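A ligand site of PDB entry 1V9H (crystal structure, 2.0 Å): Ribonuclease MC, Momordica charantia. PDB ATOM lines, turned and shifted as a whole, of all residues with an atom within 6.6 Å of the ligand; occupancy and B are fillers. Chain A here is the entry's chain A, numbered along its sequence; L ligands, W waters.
Trp 44 touches the ligand (CZ2 to O9, 3.8 Å). Leu 80 touches the ligand. CZ of Phe 87 touches C2 of the ligand, 3.5 Å away. His 90 touches the ligand. Within 4 Å of the ligand: Gln 16, His 41, Trp 44, Asn 78, Val 79, Leu 80, Arg 81, Phe 87, His 90, Glu 91, Lys 94 and His 95.
The side-chain amide oxygen (OD1) of Asn 78 lies within hydrogen-bond range of the backbone NH (N) of Arg 81 (3.0 Å). The side-chain carboxylate of Glu 91 lies within hydrogen-bond range of the indole nitrogen of Trp 44, 3.0 Å away. A ring nitrogen (NE2) of His 95 lies within hydrogen-bond range of the indole nitrogen (NE1) of Trp 44 (3.2 Å). The side-chain carboxylate of Glu 91 sits at hydrogen-bond distance from a ring nitrogen (ND1) of His 90 (3.4 Å). The side-chain amide nitrogen (ND2) of Asn 78 lies within hydrogen-bond range of the backbone carbonyl oxygen (O) of Asn 83 (3.0 Å). OD1 of Asn 78 is in hydrogen-bond range of N of Leu 80 (3.1 Å). A ring nitrogen (ND1) of His 41 sits at hydrogen-bond distance from the side-chain carboxylate (OE2) of Glu 171 (2.5 Å). The backbone carbonyl oxygen of Thr 39 lies within hydrogen-bond range of the backbone NH of Gln 16.
OD1 of Asn 78 sits at hydrogen-bond distance from N2 of the ligand, at 2.9 Å. The backbone NH (N) of Val 79 sits at hydrogen-bond distance from an oxygen (O2) of the ligand. NE2 of Gln 16 sits at hydrogen-bond distance from O2 of the ligand (2.9 Å). NH2 of Arg 81 is in hydrogen-bond range of O1 of the ligand (3.0 Å). NE2 of His 95 sits at hydrogen-bond distance from O9 of the ligand. An oxygen (O6) of the ligand lies within hydrogen-bond range of a ring nitrogen (NE2) of His 41 (2.7 Å). An oxygen (O9) of the ligand sits close to the side-chain carboxylate of Glu 91. The side-chain amino group (NZ) of Lys 94 is in salt-bridge range of an oxygen (O8) of the ligand (2.8 Å).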
ATOM      1  N   GLN A  16     -10.768   5.999 -26.605  1.00  0.00           N
ATOM      2  CA  GLN A  16     -10.353   7.348 -26.272  1.00  0.00           C
ATOM      3  C   GLN A  16     -11.276   8.411 -26.855  1.00  0.00           C
ATOM      4  O   GLN A  16     -11.911   8.189 -27.878  1.00  0.00           O
ATOM      5  CB  GLN A  16      -8.913   7.584 -26.790  1.00  0.00           C
ATOM      6  CG  GLN A  16      -8.729   7.405 -28.295  1.00  0.00           C
ATOM      7  CD  GLN A  16      -7.284   7.641 -28.733  1.00  0.00           C
ATOM      8  OE1 GLN A  16      -6.459   8.057 -27.928  1.00  0.00           O
ATOM      9  NE2 GLN A  16      -6.987   7.382 -30.006  1.00  0.00           N
ATOM     10  N   VAL A  21      -7.966  14.028 -25.980  1.00  0.00           N
ATOM     11  CA  VAL A  21      -6.633  13.533 -26.291  1.00  0.00           C
ATOM     12  C   VAL A  21      -5.854  14.585 -27.084  1.00  0.00           C
ATOM     13  O   VAL A  21      -4.675  14.840 -26.820  1.00  0.00           O
ATOM     14  CB  VAL A  21      -6.692  12.226 -27.102  1.00  0.00           C
ATOM     15  CG1 VAL A  21      -5.292  11.835 -27.581  1.00  0.00           C
ATOM     16  CG2 VAL A  21      -7.292  11.112 -26.250  1.00  0.00           C
ATOM     17  N   GLN A  25      -2.156  17.905 -26.637  1.00  0.00           N
ATOM     18  CA  GLN A  25      -1.059  17.943 -27.594  1.00  0.00           C
ATOM     19  C   GLN A  25      -0.996  19.379 -28.137  1.00  0.00           C
ATOM     20  O   GLN A  25      -1.086  19.597 -29.352  1.00  0.00           O
ATOM     21  CB  GLN A  25      -1.308  16.965 -28.737  1.00  0.00           C
ATOM     22  CG  GLN A  25      -1.449  15.513 -28.288  1.00  0.00           C
ATOM     23  CD  GLN A  25      -0.173  14.962 -27.669  1.00  0.00           C
ATOM     24  OE1 GLN A  25       0.868  14.906 -28.318  1.00  0.00           O
ATOM     25  NE2 GLN A  25      -0.257  14.533 -26.408  1.00  0.00           N
ATOM     26  N   THR A  39     -13.121   6.528 -30.086  1.00  0.00           N
ATOM     27  CA  THR A  39     -12.407   5.693 -31.035  1.00  0.00           C
ATOM     28  C   THR A  39     -11.500   4.745 -30.253  1.00  0.00           C
ATOM     29  O   THR A  39     -11.193   4.957 -29.077  1.00  0.00           O
ATOM     30  CB  THR A  39     -11.551   6.537 -32.007  1.00  0.00           C
ATOM     31  OG1 THR A  39     -10.624   7.345 -31.273  1.00  0.00           O
ATOM     32  CG2 THR A  39     -12.445   7.438 -32.862  1.00  0.00           C
ATOM     33  N   ILE A  40     -11.077   3.677 -30.913  1.00  0.00           N
ATOM     34  CA  ILE A  40     -10.236   2.664 -30.285  1.00  0.00           C
ATOM     35  C   ILE A  40      -8.817   3.136 -30.004  1.00  0.00           C
ATOM     36  O   ILE A  40      -8.166   3.708 -30.874  1.00  0.00           O
ATOM     37  CB  ILE A  40     -10.126   1.408 -31.168  1.00  0.00           C
ATOM     38  CG1 ILE A  40     -11.517   0.843 -31.456  1.00  0.00           C
ATOM     39  CG2 ILE A  40      -9.227   0.369 -30.501  1.00  0.00           C
ATOM     40  CD1 ILE A  40     -11.516  -0.244 -32.536  1.00  0.00           C
ATOM     41  N   HIS A  41      -8.331   2.889 -28.795  1.00  0.00           N
ATOM     42  CA  HIS A  41      -6.948   3.210 -28.481  1.00  0.00           C
ATOM     43  C   HIS A  41      -6.252   1.862 -28.674  1.00  0.00           C
ATOM     44  O   HIS A  41      -5.304   1.750 -29.446  1.00  0.00           O
ATOM     45  CB  HIS A  41      -6.777   3.707 -27.053  1.00  0.00           C
ATOM     46  CG  HIS A  41      -5.368   4.023 -26.684  1.00  0.00           C
ATOM     47  ND1 HIS A  41      -5.037   4.772 -25.576  1.00  0.00           N
ATOM     48  CD2 HIS A  41      -4.190   3.686 -27.282  1.00  0.00           C
ATOM     49  CE1 HIS A  41      -3.711   4.883 -25.504  1.00  0.00           C
ATOM     50  NE2 HIS A  41      -3.181   4.226 -26.520  1.00  0.00           N
ATOM     51  N   GLY A  42      -6.742   0.839 -27.976  1.00  0.00           N
ATOM     52  CA  GLY A  42      -6.158  -0.471 -28.123  1.00  0.00           C
ATOM     53  C   GLY A  42      -6.779  -1.519 -27.221  1.00  0.00           C
ATOM     54  O   GLY A  42      -7.617  -1.204 -26.358  1.00  0.00           O
ATOM     55  N   TRP A  44      -5.674  -4.138 -24.511  1.00  0.00           N
ATOM     56  CA  TRP A  44      -4.534  -4.455 -23.644  1.00  0.00           C
ATOM     57  C   TRP A  44      -4.663  -5.671 -22.738  1.00  0.00           C
ATOM     58  O   TRP A  44      -5.431  -5.664 -21.780  1.00  0.00           O
ATOM     59  CB  TRP A  44      -4.227  -3.247 -22.749  1.00  0.00           C
ATOM     60  CG  TRP A  44      -4.084  -1.922 -23.457  1.00  0.00           C
ATOM     61  CD1 TRP A  44      -3.910  -1.719 -24.796  1.00  0.00           C
ATOM     62  CD2 TRP A  44      -4.042  -0.631 -22.846  1.00  0.00           C
ATOM     63  NE1 TRP A  44      -3.744  -0.383 -25.052  1.00  0.00           N
ATOM     64  CE2 TRP A  44      -3.830   0.316 -23.876  1.00  0.00           C
ATOM     65  CE3 TRP A  44      -4.160  -0.168 -21.518  1.00  0.00           C
ATOM     66  CZ2 TRP A  44      -3.722   1.688 -23.629  1.00  0.00           C
ATOM     67  CZ3 TRP A  44      -4.060   1.199 -21.273  1.00  0.00           C
ATOM     68  CH2 TRP A  44      -3.845   2.112 -22.319  1.00  0.00           C
ATOM     69  N   PRO A  77      -8.648   5.358 -35.858  1.00  0.00           N
ATOM     70  CA  PRO A  77      -7.710   6.300 -36.461  1.00  0.00           C
ATOM     71  C   PRO A  77      -6.639   6.768 -35.483  1.00  0.00           C
ATOM     72  O   PRO A  77      -6.827   6.711 -34.260  1.00  0.00           O
ATOM     73  CB  PRO A  77      -8.606   7.461 -36.874  1.00  0.00           C
ATOM     74  CG  PRO A  77      -9.598   7.480 -35.742  1.00  0.00           C
ATOM     75  CD  PRO A  77      -9.946   6.012 -35.587  1.00  0.00           C
ATOM     76  N   ASN A  78      -5.510   7.219 -36.017  1.00  0.00           N
ATOM     77  CA  ASN A  78      -4.466   7.771 -35.176  1.00  0.00           C
ATOM     78  C   ASN A  78      -4.954   9.222 -35.066  1.00  0.00           C
ATOM     79  O   ASN A  78      -4.940   9.958 -36.055  1.00  0.00           O
ATOM     80  CB  ASN A  78      -3.123   7.737 -35.903  1.00  0.00           C
ATOM     81  CG  ASN A  78      -1.988   8.283 -35.059  1.00  0.00           C
ATOM     82  OD1 ASN A  78      -2.208   9.110 -34.174  1.00  0.00           O
ATOM     83  ND2 ASN A  78      -0.775   7.837 -35.325  1.00  0.00           N
ATOM     84  N   VAL A  79      -5.420   9.625 -33.881  1.00  0.00           N
ATOM     85  CA  VAL A  79      -5.940  10.980 -33.719  1.00  0.00           C
ATOM     86  C   VAL A  79      -4.854  12.047 -33.586  1.00  0.00           C
ATOM     87  O   VAL A  79      -5.103  13.217 -33.861  1.00  0.00           O
ATOM     88  CB  VAL A  79      -6.884  11.091 -32.485  1.00  0.00           C
ATOM     89  CG1 VAL A  79      -7.983  10.044 -32.569  1.00  0.00           C
ATOM     90  CG2 VAL A  79      -6.082  10.937 -31.203  1.00  0.00           C
ATOM     91  N   LEU A  80      -3.659  11.633 -33.190  1.00  0.00           N
ATOM     92  CA  LEU A  80      -2.555  12.563 -32.991  1.00  0.00           C
ATOM     93  C   LEU A  80      -1.766  12.876 -34.255  1.00  0.00           C
ATOM     94  O   LEU A  80      -1.330  14.006 -34.459  1.00  0.00           O
ATOM     95  CB  LEU A  80      -1.601  12.018 -31.921  1.00  0.00           C
ATOM     96  CG  LEU A  80      -2.216  11.789 -30.539  1.00  0.00           C
ATOM     97  CD1 LEU A  80      -1.151  11.263 -29.576  1.00  0.00           C
ATOM     98  CD2 LEU A  80      -2.787  13.098 -30.028  1.00  0.00           C
ATOM     99  N   ARG A  81      -1.572  11.861 -35.100  1.00  0.00           N
ATOM    100  CA  ARG A  81      -0.813  12.028 -36.329  1.00  0.00           C
ATOM    101  C   ARG A  81      -1.537  11.340 -37.486  1.00  0.00           C
ATOM    102  O   ARG A  81      -2.299  10.407 -37.281  1.00  0.00           O
ATOM    103  CB  ARG A  81       0.580  11.415 -36.175  1.00  0.00           C
ATOM    104  CG  ARG A  81       1.477  12.126 -35.186  1.00  0.00           C
ATOM    105  CD  ARG A  81       2.728  11.313 -34.892  1.00  0.00           C
ATOM    106  NE  ARG A  81       2.500  10.303 -33.868  1.00  0.00           N
ATOM    107  CZ  ARG A  81       2.345  10.583 -32.574  1.00  0.00           C
ATOM    108  NH1 ARG A  81       2.396  11.834 -32.151  1.00  0.00           N
ATOM    109  NH2 ARG A  81       2.145   9.601 -31.702  1.00  0.00           N
ATOM    110  N   ASN A  83      -1.026   8.988 -39.482  1.00  0.00           N
ATOM    111  CA  ASN A  83      -0.412   7.702 -39.824  1.00  0.00           C
ATOM    112  C   ASN A  83      -1.092   6.618 -38.986  1.00  0.00           C
ATOM    113  O   ASN A  83      -0.639   6.280 -37.897  1.00  0.00           O
ATOM    114  CB  ASN A  83       1.083   7.729 -39.530  1.00  0.00           C
ATOM    115  CG  ASN A  83       1.811   6.516 -40.097  1.00  0.00           C
ATOM    116  OD1 ASN A  83       1.214   5.446 -40.288  1.00  0.00           O
ATOM    117  ND2 ASN A  83       3.106   6.670 -40.345  1.00  0.00           N
ATOM    118  N   GLN A  86       1.011   3.231 -38.257  1.00  0.00           N
ATOM    119  CA  GLN A  86       2.029   3.365 -37.217  1.00  0.00           C
ATOM    120  C   GLN A  86       1.409   3.114 -35.851  1.00  0.00           C
ATOM    121  O   GLN A  86       2.025   2.496 -34.980  1.00  0.00           O
ATOM    122  CB  GLN A  86       2.639   4.763 -37.269  1.00  0.00           C
ATOM    123  CG  GLN A  86       3.736   5.002 -36.250  1.00  0.00           C
ATOM    124  CD  GLN A  86       4.455   6.335 -36.466  1.00  0.00           C
ATOM    125  OE1 GLN A  86       3.860   7.404 -36.344  1.00  0.00           O
ATOM    126  NE2 GLN A  86       5.735   6.258 -36.797  1.00  0.00           N
ATOM    127  N   PHE A  87       0.190   3.612 -35.662  1.00  0.00           N
ATOM    128  CA  PHE A  87      -0.529   3.466 -34.402  1.00  0.00           C
ATOM    129  C   PHE A  87      -0.930   2.000 -34.185  1.00  0.00           C
ATOM    130  O   PHE A  87      -0.722   1.449 -33.106  1.00  0.00           O
ATOM    131  CB  PHE A  87      -1.761   4.388 -34.418  1.00  0.00           C
ATOM    132  CG  PHE A  87      -2.515   4.436 -33.116  1.00  0.00           C
ATOM    133  CD1 PHE A  87      -1.855   4.275 -31.897  1.00  0.00           C
ATOM    134  CD2 PHE A  87      -3.888   4.702 -33.109  1.00  0.00           C
ATOM    135  CE1 PHE A  87      -2.561   4.376 -30.691  1.00  0.00           C
ATOM    136  CE2 PHE A  87      -4.597   4.809 -31.910  1.00  0.00           C
ATOM    137  CZ  PHE A  87      -3.932   4.643 -30.697  1.00  0.00           C
ATOM    138  N   HIS A  90       2.128  -0.079 -33.383  1.00  0.00           N
ATOM    139  CA  HIS A  90       2.585   0.121 -32.013  1.00  0.00           C
ATOM    140  C   HIS A  90       1.718  -0.633 -31.001  1.00  0.00           C
ATOM    141  O   HIS A  90       2.238  -1.272 -30.085  1.00  0.00           O
ATOM    142  CB  HIS A  90       2.584   1.614 -31.663  1.00  0.00           C
ATOM    143  CG  HIS A  90       2.934   1.890 -30.229  1.00  0.00           C
ATOM    144  ND1 HIS A  90       1.982   2.140 -29.270  1.00  0.00           N
ATOM    145  CD2 HIS A  90       4.127   1.912 -29.596  1.00  0.00           C
ATOM    146  CE1 HIS A  90       2.572   2.307 -28.100  1.00  0.00           C
ATOM    147  NE2 HIS A  90       3.871   2.167 -28.272  1.00  0.00           N
ATOM    148  N   GLU A  91       0.401  -0.564 -31.169  1.00  0.00           N
ATOM    149  CA  GLU A  91      -0.496  -1.232 -30.237  1.00  0.00           C
ATOM    150  C   GLU A  91      -0.342  -2.748 -30.321  1.00  0.00           C
ATOM    151  O   GLU A  91      -0.433  -3.440 -29.294  1.00  0.00           O
ATOM    152  CB  GLU A  91      -1.950  -0.825 -30.517  1.00  0.00           C
ATOM    153  CG  GLU A  91      -2.256   0.624 -30.120  1.00  0.00           C
ATOM    154  CD  GLU A  91      -2.088   0.874 -28.629  1.00  0.00           C
ATOM    155  OE1 GLU A  91      -2.787   0.221 -27.838  1.00  0.00           O
ATOM    156  OE2 GLU A  91      -1.256   1.722 -28.249  1.00  0.00           O
ATOM    157  N   LYS A  94       3.264  -3.568 -28.683  1.00  0.00           N
ATOM    158  CA  LYS A  94       3.264  -3.344 -27.247  1.00  0.00           C
ATOM    159  C   LYS A  94       2.228  -4.152 -26.466  1.00  0.00           C
ATOM    160  O   LYS A  94       2.516  -4.629 -25.367  1.00  0.00           O
ATOM    161  CB  LYS A  94       3.067  -1.852 -26.964  1.00  0.00           C
ATOM    162  CG  LYS A  94       3.140  -1.498 -25.484  1.00  0.00           C
ATOM    163  CD  LYS A  94       3.159   0.010 -25.267  1.00  0.00           C
ATOM    164  CE  LYS A  94       3.240   0.353 -23.786  1.00  0.00           C
ATOM    165  NZ  LYS A  94       3.377   1.820 -23.578  1.00  0.00           N
ATOM    166  N   HIS A  95       1.046  -4.335 -27.036  1.00  0.00           N
ATOM    167  CA  HIS A  95      -0.028  -5.028 -26.334  1.00  0.00           C
ATOM    168  C   HIS A  95      -0.489  -6.359 -26.948  1.00  0.00           C
ATOM    169  O   HIS A  95      -0.547  -7.376 -26.254  1.00  0.00           O
ATOM    170  CB  HIS A  95      -1.230  -4.086 -26.220  1.00  0.00           C
ATOM    171  CG  HIS A  95      -0.934  -2.802 -25.503  1.00  0.00           C
ATOM    172  ND1 HIS A  95      -0.758  -2.736 -24.131  1.00  0.00           N
ATOM    173  CD2 HIS A  95      -0.769  -1.540 -25.959  1.00  0.00           C
ATOM    174  CE1 HIS A  95      -0.513  -1.486 -23.779  1.00  0.00           C
ATOM    175  NE2 HIS A  95      -0.521  -0.738 -24.871  1.00  0.00           N
ATOM    176  N   GLU A 171     -10.264   8.609 -21.563  1.00  0.00           N
ATOM    177  CA  GLU A 171     -10.498   7.239 -22.022  1.00  0.00           C
ATOM    178  C   GLU A 171     -11.514   6.500 -21.161  1.00  0.00           C
ATOM    179  O   GLU A 171     -11.694   6.782 -19.979  1.00  0.00           O
ATOM    180  CB  GLU A 171      -9.186   6.457 -22.024  1.00  0.00           C
ATOM    181  CG  GLU A 171      -8.078   7.117 -22.823  1.00  0.00           C
ATOM    182  CD  GLU A 171      -6.803   6.290 -22.850  1.00  0.00           C
ATOM    183  OE1 GLU A 171      -6.465   5.690 -21.807  1.00  0.00           O
ATOM    184  OE2 GLU A 171      -6.145   6.244 -23.910  1.00  0.00           O
HETATM  185  N1  LIG L   1      -1.072   7.490 -29.569  1.00  0.00           N
HETATM  186  C1  LIG L   1      -1.149   7.680 -30.964  1.00  0.00           C
HETATM  187  N2  LIG L   1      -2.401   7.962 -31.465  1.00  0.00           N
HETATM  188  C2  LIG L   1      -3.591   8.076 -30.726  1.00  0.00           C
HETATM  189  C3  LIG L   1      -3.436   7.873 -29.303  1.00  0.00           C
HETATM  190  C4  LIG L   1      -2.241   7.596 -28.790  1.00  0.00           C
HETATM  191  O1  LIG L   1      -0.138   7.591 -31.656  1.00  0.00           O
HETATM  192  O2  LIG L   1      -4.608   8.341 -31.328  1.00  0.00           O
HETATM  193  C5  LIG L   1       0.263   7.192 -29.002  1.00  0.00           C
HETATM  194  C6  LIG L   1       0.816   8.191 -27.994  1.00  0.00           C
HETATM  195  O3  LIG L   1       1.504   9.295 -28.613  1.00  0.00           O
HETATM  196  C7  LIG L   1       1.686   7.358 -27.031  1.00  0.00           C
HETATM  197  C8  LIG L   1       1.025   5.986 -27.103  1.00  0.00           C
HETATM  198  O4  LIG L   1       3.096   7.411 -27.408  1.00  0.00           O
HETATM  199  O5  LIG L   1       0.365   5.909 -28.402  1.00  0.00           O
HETATM  200  C9  LIG L   1      -0.037   5.624 -26.067  1.00  0.00           C
HETATM  201  O6  LIG L   1      -0.489   4.250 -26.120  1.00  0.00           O
HETATM  202  P1  LIG L   1       0.159   3.090 -25.192  1.00  0.00           P
HETATM  203  O7  LIG L   1       0.095   3.248 -23.708  1.00  0.00           O
HETATM  204  O8  LIG L   1       1.607   2.934 -25.474  1.00  0.00           O
HETATM  205  O9  LIG L   1      -0.578   1.742 -25.802  1.00  0.00           O
HETATM  206  O   HOH W   1      -2.521   7.993 -25.477  1.00  0.00           O
HETATM  207  O   HOH W   2      -1.710   5.432 -23.116  1.00  0.00           O
HETATM  208  O   HOH W   3      -0.030   1.189 -21.680  1.00  0.00           O
HETATM  209  O   HOH W   4       1.916   4.853 -22.072  1.00  0.00           O
HETATM  210  O   HOH W   5       1.800   5.684 -32.947  1.00  0.00           O
HETATM  211  O   HOH W   6       1.707  11.174 -26.014  1.00  0.00           O
